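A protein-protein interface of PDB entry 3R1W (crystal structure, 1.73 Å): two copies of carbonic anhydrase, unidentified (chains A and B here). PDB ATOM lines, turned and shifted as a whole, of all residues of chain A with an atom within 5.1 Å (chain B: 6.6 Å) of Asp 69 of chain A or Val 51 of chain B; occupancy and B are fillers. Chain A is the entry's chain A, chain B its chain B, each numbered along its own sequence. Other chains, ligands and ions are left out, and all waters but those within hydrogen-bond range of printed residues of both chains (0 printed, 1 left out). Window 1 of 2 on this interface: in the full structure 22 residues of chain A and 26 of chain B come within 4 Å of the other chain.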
ATOM      1  N   TRP A  47     -24.277  -4.318 -11.611  1.00  0.00           N
ATOM      2  CA  TRP A  47     -23.821  -4.723 -10.282  1.00  0.00           C
ATOM      3  C   TRP A  47     -24.803  -4.290  -9.181  1.00  0.00           C
ATOM      4  O   TRP A  47     -25.781  -3.589  -9.464  1.00  0.00           O
ATOM      5  CB  TRP A  47     -22.378  -4.230 -10.074  1.00  0.00           C
ATOM      6  CG  TRP A  47     -21.484  -4.925 -11.075  1.00  0.00           C
ATOM      7  CD1 TRP A  47     -21.218  -4.533 -12.364  1.00  0.00           C
ATOM      8  CD2 TRP A  47     -20.836  -6.195 -10.901  1.00  0.00           C
ATOM      9  NE1 TRP A  47     -20.407  -5.464 -12.985  1.00  0.00           N
ATOM     10  CE2 TRP A  47     -20.170  -6.495 -12.113  1.00  0.00           C
ATOM     11  CE3 TRP A  47     -20.739  -7.095  -9.835  1.00  0.00           C
ATOM     12  CZ2 TRP A  47     -19.409  -7.650 -12.276  1.00  0.00           C
ATOM     13  CZ3 TRP A  47     -19.999  -8.244 -10.005  1.00  0.00           C
ATOM     14  CH2 TRP A  47     -19.334  -8.513 -11.217  1.00  0.00           C
ATOM     15  N   PRO A  48     -24.582  -4.746  -7.937  1.00  0.00           N
ATOM     16  CA  PRO A  48     -25.578  -4.472  -6.892  1.00  0.00           C
ATOM     17  C   PRO A  48     -26.038  -3.013  -6.784  1.00  0.00           C
ATOM     18  O   PRO A  48     -25.232  -2.077  -6.807  1.00  0.00           O
ATOM     19  CB  PRO A  48     -24.863  -4.914  -5.613  1.00  0.00           C
ATOM     20  CG  PRO A  48     -24.017  -6.060  -6.083  1.00  0.00           C
ATOM     21  CD  PRO A  48     -23.482  -5.594  -7.432  1.00  0.00           C
ATOM     22  N   LEU A  49     -27.355  -2.844  -6.704  1.00  0.00           N
ATOM     23  CA  LEU A  49     -27.974  -1.558  -6.404  1.00  0.00           C
ATOM     24  C   LEU A  49     -27.727  -0.473  -7.463  1.00  0.00           C
ATOM     25  O   LEU A  49     -27.720   0.718  -7.159  1.00  0.00           O
ATOM     26  CB  LEU A  49     -27.572  -1.087  -4.992  1.00  0.00           C
ATOM     27  CG  LEU A  49     -27.871  -2.085  -3.862  1.00  0.00           C
ATOM     28  CD1 LEU A  49     -27.518  -1.519  -2.483  1.00  0.00           C
ATOM     29  CD2 LEU A  49     -29.329  -2.495  -3.881  1.00  0.00           C
ATOM     30  N   ALA A  50     -27.552  -0.894  -8.715  1.00  0.00           N
ATOM     31  CA  ALA A  50     -27.521   0.038  -9.839  1.00  0.00           C
ATOM     32  C   ALA A  50     -28.933   0.154 -10.420  1.00  0.00           C
ATOM     33  O   ALA A  50     -29.717  -0.790 -10.333  1.00  0.00           O
ATOM     34  CB  ALA A  50     -26.559  -0.460 -10.905  1.00  0.00           C
ATOM     35  N   VAL A  67     -21.718  -1.915 -15.473  1.00  0.00           N
ATOM     36  CA  VAL A  67     -22.403  -0.802 -14.831  1.00  0.00           C
ATOM     37  C   VAL A  67     -22.302  -1.083 -13.342  1.00  0.00           C
ATOM     38  O   VAL A  67     -23.058  -1.889 -12.811  1.00  0.00           O
ATOM     39  CB  VAL A  67     -23.892  -0.716 -15.259  1.00  0.00           C
ATOM     40  CG1 VAL A  67     -24.619   0.419 -14.519  1.00  0.00           C
ATOM     41  CG2 VAL A  67     -24.019  -0.520 -16.788  1.00  0.00           C
ATOM     42  N   GLN A  68     -21.355  -0.435 -12.670  1.00  0.00           N
ATOM     43  CA  GLN A  68     -20.996  -0.853 -11.315  1.00  0.00           C
ATOM     44  C   GLN A  68     -21.921  -0.342 -10.205  1.00  0.00           C
ATOM     45  O   GLN A  68     -22.856   0.439 -10.452  1.00  0.00           O
ATOM     46  CB  GLN A  68     -19.524  -0.547 -11.029  1.00  0.00           C
ATOM     47  CG  GLN A  68     -18.602  -1.344 -11.949  1.00  0.00           C
ATOM     48  CD  GLN A  68     -17.144  -0.976 -11.799  1.00  0.00           C
ATOM     49  OE1 GLN A  68     -16.751  -0.308 -10.841  1.00  0.00           O
ATOM     50  NE2 GLN A  68     -16.330  -1.402 -12.756  1.00  0.00           N
ATOM     51  N   ASP A  69     -21.654  -0.832  -8.995  1.00  0.00           N
ATOM     52  CA  ASP A  69     -22.552  -0.715  -7.846  1.00  0.00           C
ATOM     53  C   ASP A  69     -23.032   0.703  -7.591  1.00  0.00           C
ATOM     54  O   ASP A  69     -22.236   1.627  -7.502  1.00  0.00           O
ATOM     55  CB  ASP A  69     -21.871  -1.231  -6.568  1.00  0.00           C
ATOM     56  CG  ASP A  69     -20.925  -2.393  -6.828  1.00  0.00           C
ATOM     57  OD1 ASP A  69     -19.931  -2.202  -7.566  1.00  0.00           O
ATOM     58  OD2 ASP A  69     -21.162  -3.488  -6.274  1.00  0.00           O
ATOM     59  N   GLY A  70     -24.347   0.864  -7.450  1.00  0.00           N
ATOM     60  CA  GLY A  70     -24.913   2.143  -7.080  1.00  0.00           C
ATOM     61  C   GLY A  70     -24.962   3.169  -8.187  1.00  0.00           C
ATOM     62  O   GLY A  70     -25.301   4.322  -7.931  1.00  0.00           O
ATOM     63  N   SER A  71     -24.641   2.761  -9.417  1.00  0.00           N
ATOM     64  CA  SER A  71     -24.733   3.682 -10.554  1.00  0.00           C
ATOM     65  C   SER A  71     -26.195   3.949 -10.884  1.00  0.00           C
ATOM     66  O   SER A  71     -27.046   3.101 -10.651  1.00  0.00           O
ATOM     67  CB  SER A  71     -24.019   3.119 -11.780  1.00  0.00           C
ATOM     68  OG  SER A  71     -22.610   3.156 -11.608  1.00  0.00           O
ATOM     69  N   GLY A  97     -17.855   3.173 -13.477  1.00  0.00           N
ATOM     70  CA  GLY A  97     -17.477   2.997 -12.083  1.00  0.00           C
ATOM     71  C   GLY A  97     -18.617   3.101 -11.084  1.00  0.00           C
ATOM     72  O   GLY A  97     -19.712   3.579 -11.403  1.00  0.00           O
ATOM     73  N   HIS A  98     -18.356   2.633  -9.864  1.00  0.00           N
ATOM     74  CA  HIS A  98     -19.350   2.667  -8.791  1.00  0.00           C
ATOM     75  C   HIS A  98     -19.969   4.053  -8.628  1.00  0.00           C
ATOM     76  O   HIS A  98     -19.281   5.070  -8.738  1.00  0.00           O
ATOM     77  CB  HIS A  98     -18.734   2.268  -7.444  1.00  0.00           C
ATOM     78  CG  HIS A  98     -17.734   1.159  -7.526  1.00  0.00           C
ATOM     79  ND1 HIS A  98     -18.089  -0.168  -7.463  1.00  0.00           N
ATOM     80  CD2 HIS A  98     -16.382   1.189  -7.609  1.00  0.00           C
ATOM     81  CE1 HIS A  98     -16.997  -0.916  -7.538  1.00  0.00           C
ATOM     82  NE2 HIS A  98     -15.953  -0.117  -7.629  1.00  0.00           N
ATOM     83  N   GLN A  99     -21.271   4.085  -8.369  1.00  0.00           N
ATOM     84  CA  GLN A  99     -21.954   5.339  -8.072  1.00  0.00           C
ATOM     85  C   GLN A  99     -21.853   6.377  -9.196  1.00  0.00           C
ATOM     86  O   GLN A  99     -21.971   7.583  -8.947  1.00  0.00           O
ATOM     87  CB  GLN A  99     -21.418   5.926  -6.761  1.00  0.00           C
ATOM     88  CG  GLN A  99     -21.614   5.016  -5.551  1.00  0.00           C
ATOM     89  CD  GLN A  99     -21.063   5.636  -4.275  1.00  0.00           C
ATOM     90  OE1 GLN A  99     -20.202   6.508  -4.328  1.00  0.00           O
ATOM     91  NE2 GLN A  99     -21.559   5.187  -3.126  1.00  0.00           N
ATOM     92  N   SER B  32     -29.303  -4.085   2.269  1.00  0.00           N
ATOM     93  CA  SER B  32     -27.893  -3.924   1.949  1.00  0.00           C
ATOM     94  C   SER B  32     -27.359  -5.203   1.296  1.00  0.00           C
ATOM     95  O   SER B  32     -28.037  -6.234   1.275  1.00  0.00           O
ATOM     96  CB  SER B  32     -27.088  -3.566   3.192  1.00  0.00           C
ATOM     97  OG  SER B  32     -27.074  -4.647   4.098  1.00  0.00           O
ATOM     98  N   VAL B  33     -26.155  -5.129   0.745  1.00  0.00           N
ATOM     99  CA  VAL B  33     -25.572  -6.273   0.042  1.00  0.00           C
ATOM    100  C   VAL B  33     -24.118  -6.463   0.448  1.00  0.00           C
ATOM    101  O   VAL B  33     -23.267  -5.633   0.142  1.00  0.00           O
ATOM    102  CB  VAL B  33     -25.661  -6.111  -1.493  1.00  0.00           C
ATOM    103  CG1 VAL B  33     -24.860  -7.205  -2.198  1.00  0.00           C
ATOM    104  CG2 VAL B  33     -27.117  -6.140  -1.939  1.00  0.00           C
ATOM    105  N   ILE B  34     -23.838  -7.560   1.145  1.00  0.00           N
ATOM    106  CA  ILE B  34     -22.475  -7.857   1.575  1.00  0.00           C
ATOM    107  C   ILE B  34     -22.034  -9.156   0.927  1.00  0.00           C
ATOM    108  O   ILE B  34     -22.722 -10.173   1.033  1.00  0.00           O
ATOM    109  CB  ILE B  34     -22.384  -7.990   3.106  1.00  0.00           C
ATOM    110  CG1 ILE B  34     -22.891  -6.707   3.779  1.00  0.00           C
ATOM    111  CG2 ILE B  34     -20.946  -8.259   3.531  1.00  0.00           C
ATOM    112  CD1 ILE B  34     -22.828  -6.742   5.323  1.00  0.00           C
ATOM    113  N   ILE B  35     -20.892  -9.118   0.251  1.00  0.00           N
ATOM    114  CA  ILE B  35     -20.452 -10.253  -0.559  1.00  0.00           C
ATOM    115  C   ILE B  35     -19.057 -10.736  -0.186  1.00  0.00           C
ATOM    116  O   ILE B  35     -18.098  -9.969  -0.214  1.00  0.00           O
ATOM    117  CB  ILE B  35     -20.460  -9.912  -2.067  1.00  0.00           C
ATOM    118  CG1 ILE B  35     -21.900  -9.720  -2.564  1.00  0.00           C
ATOM    119  CG2 ILE B  35     -19.755 -11.018  -2.888  1.00  0.00           C
ATOM    120  CD1 ILE B  35     -21.999  -9.039  -3.938  1.00  0.00           C
ATOM    121  N   VAL B  46     -24.713  -1.816   9.154  1.00  0.00           N
ATOM    122  CA  VAL B  46     -24.700  -1.560   7.728  1.00  0.00           C
ATOM    123  C   VAL B  46     -26.121  -1.216   7.336  1.00  0.00           C
ATOM    124  O   VAL B  46     -27.039  -2.003   7.540  1.00  0.00           O
ATOM    125  CB  VAL B  46     -24.200  -2.769   6.935  1.00  0.00           C
ATOM    126  CG1 VAL B  46     -24.160  -2.427   5.448  1.00  0.00           C
ATOM    127  CG2 VAL B  46     -22.802  -3.184   7.419  1.00  0.00           C
ATOM    128  N   TRP B  47     -26.276  -0.024   6.770  1.00  0.00           N
ATOM    129  CA  TRP B  47     -27.567   0.647   6.660  1.00  0.00           C
ATOM    130  C   TRP B  47     -28.190   0.467   5.275  1.00  0.00           C
ATOM    131  O   TRP B  47     -27.563  -0.115   4.389  1.00  0.00           O
ATOM    132  CB  TRP B  47     -27.374   2.115   7.051  1.00  0.00           C
ATOM    133  CG  TRP B  47     -26.978   2.177   8.490  1.00  0.00           C
ATOM    134  CD1 TRP B  47     -25.700   2.115   9.003  1.00  0.00           C
ATOM    135  CD2 TRP B  47     -27.859   2.222   9.617  1.00  0.00           C
ATOM    136  NE1 TRP B  47     -25.743   2.151  10.377  1.00  0.00           N
ATOM    137  CE2 TRP B  47     -27.054   2.216  10.778  1.00  0.00           C
ATOM    138  CE3 TRP B  47     -29.253   2.283   9.756  1.00  0.00           C
ATOM    139  CZ2 TRP B  47     -27.599   2.273  12.060  1.00  0.00           C
ATOM    140  CZ3 TRP B  47     -29.792   2.336  11.025  1.00  0.00           C
ATOM    141  CH2 TRP B  47     -28.965   2.338  12.164  1.00  0.00           C
ATOM    142  N   LEU B  49     -29.350  -0.100   1.677  1.00  0.00           N
ATOM    143  CA  LEU B  49     -28.831   0.082   0.324  1.00  0.00           C
ATOM    144  C   LEU B  49     -27.332   0.399   0.274  1.00  0.00           C
ATOM    145  O   LEU B  49     -26.874   1.086  -0.643  1.00  0.00           O
ATOM    146  CB  LEU B  49     -29.647   1.137  -0.428  1.00  0.00           C
ATOM    147  CG  LEU B  49     -31.161   0.876  -0.433  1.00  0.00           C
ATOM    148  CD1 LEU B  49     -31.913   1.946  -1.231  1.00  0.00           C
ATOM    149  CD2 LEU B  49     -31.473  -0.511  -0.986  1.00  0.00           C
ATOM    150  N   ALA B  50     -26.578  -0.097   1.255  1.00  0.00           N
ATOM    151  CA  ALA B  50     -25.115  -0.065   1.193  1.00  0.00           C
ATOM    152  C   ALA B  50     -24.575  -1.351   0.560  1.00  0.00           C
ATOM    153  O   ALA B  50     -25.199  -2.415   0.657  1.00  0.00           O
ATOM    154  CB  ALA B  50     -24.510   0.133   2.576  1.00  0.00           C
ATOM    155  N   VAL B  51     -23.403  -1.248  -0.063  1.00  0.00           N
ATOM    156  CA  VAL B  51     -22.755  -2.395  -0.686  1.00  0.00           C
ATOM    157  C   VAL B  51     -21.353  -2.559  -0.128  1.00  0.00           C
ATOM    158  O   VAL B  51     -20.582  -1.599  -0.088  1.00  0.00           O
ATOM    159  CB  VAL B  51     -22.665  -2.230  -2.227  1.00  0.00           C
ATOM    160  CG1 VAL B  51     -21.946  -3.430  -2.856  1.00  0.00           C
ATOM    161  CG2 VAL B  51     -24.058  -2.073  -2.817  1.00  0.00           C
ATOM    162  N   ILE B  52     -21.032  -3.771   0.323  1.00  0.00           N
ATOM    163  CA  ILE B  52     -19.668  -4.105   0.720  1.00  0.00           C
ATOM    164  C   ILE B  52     -19.264  -5.364  -0.056  1.00  0.00           C
ATOM    165  O   ILE B  52     -19.674  -6.480   0.279  1.00  0.00           O
ATOM    166  CB  ILE B  52     -19.553  -4.343   2.247  1.00  0.00           C
ATOM    167  CG1 ILE B  52     -20.272  -3.235   3.026  1.00  0.00           C
ATOM    168  CG2 ILE B  52     -18.086  -4.394   2.666  1.00  0.00           C
ATOM    169  CD1 ILE B  52     -20.229  -3.440   4.530  1.00  0.00           C
ATOM    170  N   ARG B  53     -18.488  -5.166  -1.114  1.00  0.00           N
ATOM    171  CA  ARG B  53     -18.229  -6.241  -2.075  1.00  0.00           C
ATOM    172  C   ARG B  53     -16.781  -6.732  -1.979  1.00  0.00           C
ATOM    173  O   ARG B  53     -15.865  -6.142  -2.554  1.00  0.00           O
ATOM    174  CB  ARG B  53     -18.605  -5.803  -3.504  1.00  0.00           C
ATOM    175  CG  ARG B  53     -18.337  -6.877  -4.581  1.00  0.00           C
ATOM    176  CD  ARG B  53     -19.221  -6.755  -5.838  1.00  0.00           C
ATOM    177  NE  ARG B  53     -19.032  -5.526  -6.607  1.00  0.00           N
ATOM    178  CZ  ARG B  53     -18.146  -5.363  -7.587  1.00  0.00           C
ATOM    179  NH1 ARG B  53     -17.319  -6.352  -7.914  1.00  0.00           N
ATOM    180  NH2 ARG B  53     -18.075  -4.199  -8.231  1.00  0.00           N
ATOM    181  N   VAL B  67     -21.637   1.773   8.404  1.00  0.00           N
ATOM    182  CA  VAL B  67     -21.524   1.945   6.966  1.00  0.00           C
ATOM    183  C   VAL B  67     -22.895   2.428   6.518  1.00  0.00           C
ATOM    184  O   VAL B  67     -23.821   1.639   6.405  1.00  0.00           O
ATOM    185  CB  VAL B  67     -21.196   0.612   6.272  1.00  0.00           C
ATOM    186  CG1 VAL B  67     -21.101   0.802   4.754  1.00  0.00           C
ATOM    187  CG2 VAL B  67     -19.894   0.036   6.830  1.00  0.00           C
ATOM    188  N   GLN B  68     -23.030   3.729   6.284  1.00  0.00           N
ATOM    189  CA  GLN B  68     -24.359   4.320   6.126  1.00  0.00           C
ATOM    190  C   GLN B  68     -24.973   4.236   4.727  1.00  0.00           C
ATOM    191  O   GLN B  68     -24.333   3.809   3.759  1.00  0.00           O
ATOM    192  CB  GLN B  68     -24.374   5.753   6.666  1.00  0.00           C
ATOM    193  CG  GLN B  68     -24.103   5.776   8.169  1.00  0.00           C
ATOM    194  CD  GLN B  68     -23.967   7.178   8.719  1.00  0.00           C
ATOM    195  OE1 GLN B  68     -24.275   8.159   8.038  1.00  0.00           O
ATOM    196  NE2 GLN B  68     -23.489   7.283   9.955  1.00  0.00           N
ATOM    197  N   GLY B  70     -26.472   3.745   1.274  1.00  0.00           N
ATOM    198  CA  GLY B  70     -26.037   4.038  -0.075  1.00  0.00           C
ATOM    199  C   GLY B  70     -24.530   4.068  -0.262  1.00  0.00           C
ATOM    200  O   GLY B  70     -24.062   4.358  -1.360  1.00  0.00           O
ATOM    201  N   SER B  71     -23.769   3.754   0.787  1.00  0.00           N
ATOM    202  CA  SER B  71     -22.306   3.690   0.658  1.00  0.00           C
ATOM    203  C   SER B  71     -21.903   2.481  -0.176  1.00  0.00           C
ATOM    204  O   SER B  71     -22.617   1.473  -0.216  1.00  0.00           O
ATOM    205  CB  SER B  71     -21.628   3.612   2.034  1.00  0.00           C
ATOM    206  OG  SER B  71     -21.846   4.792   2.794  1.00  0.00           O
ATOM    207  N   VAL B  72     -20.764   2.590  -0.855  1.00  0.00           N
ATOM    208  CA  VAL B  72     -20.186   1.458  -1.569  1.00  0.00           C
ATOM    209  C   VAL B  72     -18.747   1.285  -1.093  1.00  0.00           C
ATOM    210  O   VAL B  72     -17.948   2.230  -1.131  1.00  0.00           O
ATOM    211  CB  VAL B  72     -20.239   1.638  -3.106  1.00  0.00           C
ATOM    212  CG1 VAL B  72     -19.357   0.599  -3.817  1.00  0.00           C
ATOM    213  CG2 VAL B  72     -21.682   1.529  -3.605  1.00  0.00           C
ATOM    214  N   LEU B  73     -18.444   0.086  -0.597  1.00  0.00           N
ATOM    215  CA  LEU B  73     -17.090  -0.268  -0.174  1.00  0.00           C
ATOM    216  C   LEU B  73     -16.575  -1.363  -1.092  1.00  0.00           C
ATOM    217  O   LEU B  73     -17.209  -2.404  -1.233  1.00  0.00           O
ATOM    218  CB  LEU B  73     -17.077  -0.793   1.256  1.00  0.00           C
ATOM    219  CG  LEU B  73     -17.770  -0.050   2.402  1.00  0.00           C
ATOM    220  CD1 LEU B  73     -17.159  -0.432   3.762  1.00  0.00           C
ATOM    221  CD2 LEU B  73     -17.833   1.451   2.216  1.00  0.00           C
ATOM    222  N   HIS B  74     -15.424  -1.138  -1.711  1.00  0.00           N
ATOM    223  CA  HIS B  74     -14.890  -2.127  -2.629  1.00  0.00           C
ATOM    224  C   HIS B  74     -13.363  -2.088  -2.617  1.00  0.00           C
ATOM    225  O   HIS B  74     -12.745  -1.377  -1.824  1.00  0.00           O
ATOM    226  CB  HIS B  74     -15.472  -1.927  -4.042  1.00  0.00           C
ATOM    227  CG  HIS B  74     -15.252  -3.095  -4.957  1.00  0.00           C
ATOM    228  ND1 HIS B  74     -14.731  -2.964  -6.227  1.00  0.00           N
ATOM    229  CD2 HIS B  74     -15.467  -4.422  -4.775  1.00  0.00           C
ATOM    230  CE1 HIS B  74     -14.634  -4.156  -6.790  1.00  0.00           C
ATOM    231  NE2 HIS B  74     -15.075  -5.058  -5.930  1.00  0.00           N
ATOM    232  N   MET B 101     -17.854   6.507  -0.688  1.00  0.00           N
ATOM    233  CA  MET B 101     -17.246   5.612  -1.657  1.00  0.00           C
ATOM    234  C   MET B 101     -15.846   5.307  -1.175  1.00  0.00           C
ATOM    235  O   MET B 101     -14.959   6.160  -1.269  1.00  0.00           O
ATOM    236  CB  MET B 101     -17.152   6.297  -3.020  1.00  0.00           C
ATOM    237  CG  MET B 101     -16.460   5.471  -4.102  1.00  0.00           C
ATOM    238  SD  MET B 101     -17.449   4.103  -4.728  1.00  0.00           S
ATOM    239  CE  MET B 101     -16.408   2.745  -4.210  1.00  0.00           C
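The side-chain sulfur (SD) of Met 101 of chain B sits close to the side-chain amide oxygen (OE1) of Gln 99 of chain A, 3.7 Å away. The side-chain carboxylate of Asp 69 of chain A is in salt-bridge range of the guanidinium group of Arg 53 of chain B (2.8 Å). A ring nitrogen (NE2) of His 98 of chain A sits close to a ring nitrogen (ND1) of His 74 of chain B (3.4 Å). The backbone carbonyl oxygen (O) of Gly 70 of chain B is in hydrogen-bond range of the side-chain amide nitrogen (NE2) of Gln 99 of chain A.
Printed residues of chain B that touch a printed residue of chain A: Leu 49, Val 51, Arg 53, Gly 70, Val 72, His 74 and Met 101. Of the 12 printed residues of chain A, 5 touch a printed residue of chain B. Hydrophobic or aromatic side chains of chain A that line the printed part of chain B: Trp 47, Leu 49 and His 98. Among the printed residues, Asp or Glu carboxylates within 4 Å of a Lys or Arg side-chain nitrogen of the other chain: Asp 69 of chain A with Arg 53 of chain B.
O of Val 51 of chain B sits at hydrogen-bond distance from N of Leu 73 of chain B, at 2.8 Å. The backbone carbonyl oxygen of Leu 73 of chain B is in hydrogen-bond range of the backbone NH of Arg 53 of chain B, at 3.0 Å. The backbone NH (N) of Val 51 of chain B sits at hydrogen-bond distance from the backbone carbonyl oxygen (O) of Ser 71 of chain B, at 2.8 Å. The guanidinium group of Arg 53 of chain B lies within hydrogen-bond range of a ring nitrogen (NE2) of His 74 of chain B, at 3.3 Å. The side-chain amide oxygen (OE1) of Gln 68 of chain A lies within hydrogen-bond range of a ring nitrogen (NE2) of His 98 of chain A (3.3 Å). O of Val 67 of chain A sits at hydrogen-bond distance from N of Trp 47 of chain A (3.0 Å).
Leu 49 of chain A touches its own counterpart, Leu 49 of chain B. Positions printed for both chains: 47, 49, 50, 67, 68, 70 and 71. Of the 13 pairs that touch across the chains among the printed residues, 1 has its exchanged pair printed and touching as well.
Of chain B, only Val 51 (3.5 Å), Arg 53 (2.8 Å) and Val 72 (3.9 Å) come within 4 Å of Asp 69 of chain A. Of chain A, only Leu 49 and Asp 69 come within 4 Å of Val 51 of chain B. Of the printed residues of chain A, Arg 53 of chain B touches Trp 47 (3.8 Å), Asp 69 (2.8 Å) and His 98 (3.5 Å). Printed residues of chain A within 4 Å of Met 101 of chain B: His 98 (3.5 Å) and Gln 99 (3.3 Å). Of the printed residues of chain A, Gly 70 of chain B touches Gln 99 (3.2 Å). Val 46 of chain B touches none of the printed residues of chain A. Ala 50 of chain A touches none of the printed residues of chain B. The nearest residue of chain B that does not touch Asp 69 of chain A is His 74 of chain B (5.4 Å).
Among the printed residues, merely in contact across the chains: Leu 49 of chain A with Leu 49 of chain B (3.3 Å), Asp 69 of chain A with Val 51 of chain B (3.5 Å), Leu 49 of chain A with Val 51 of chain B (3.5 Å), His 98 of chain A with Met 101 of chain B (3.5 Å), His 98 of chain A with Arg 53 of chain B (3.5 Å), Gln 99 of chain A with Val 72 of chain B (3.5 Å), Trp 47 of chain A with Arg 53 of chain B (3.8 Å), His 98 of chain A with Val 72 of chain B (3.9 Å) and Asp 69 of chain A with Val 72 of chain B (3.9 Å).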
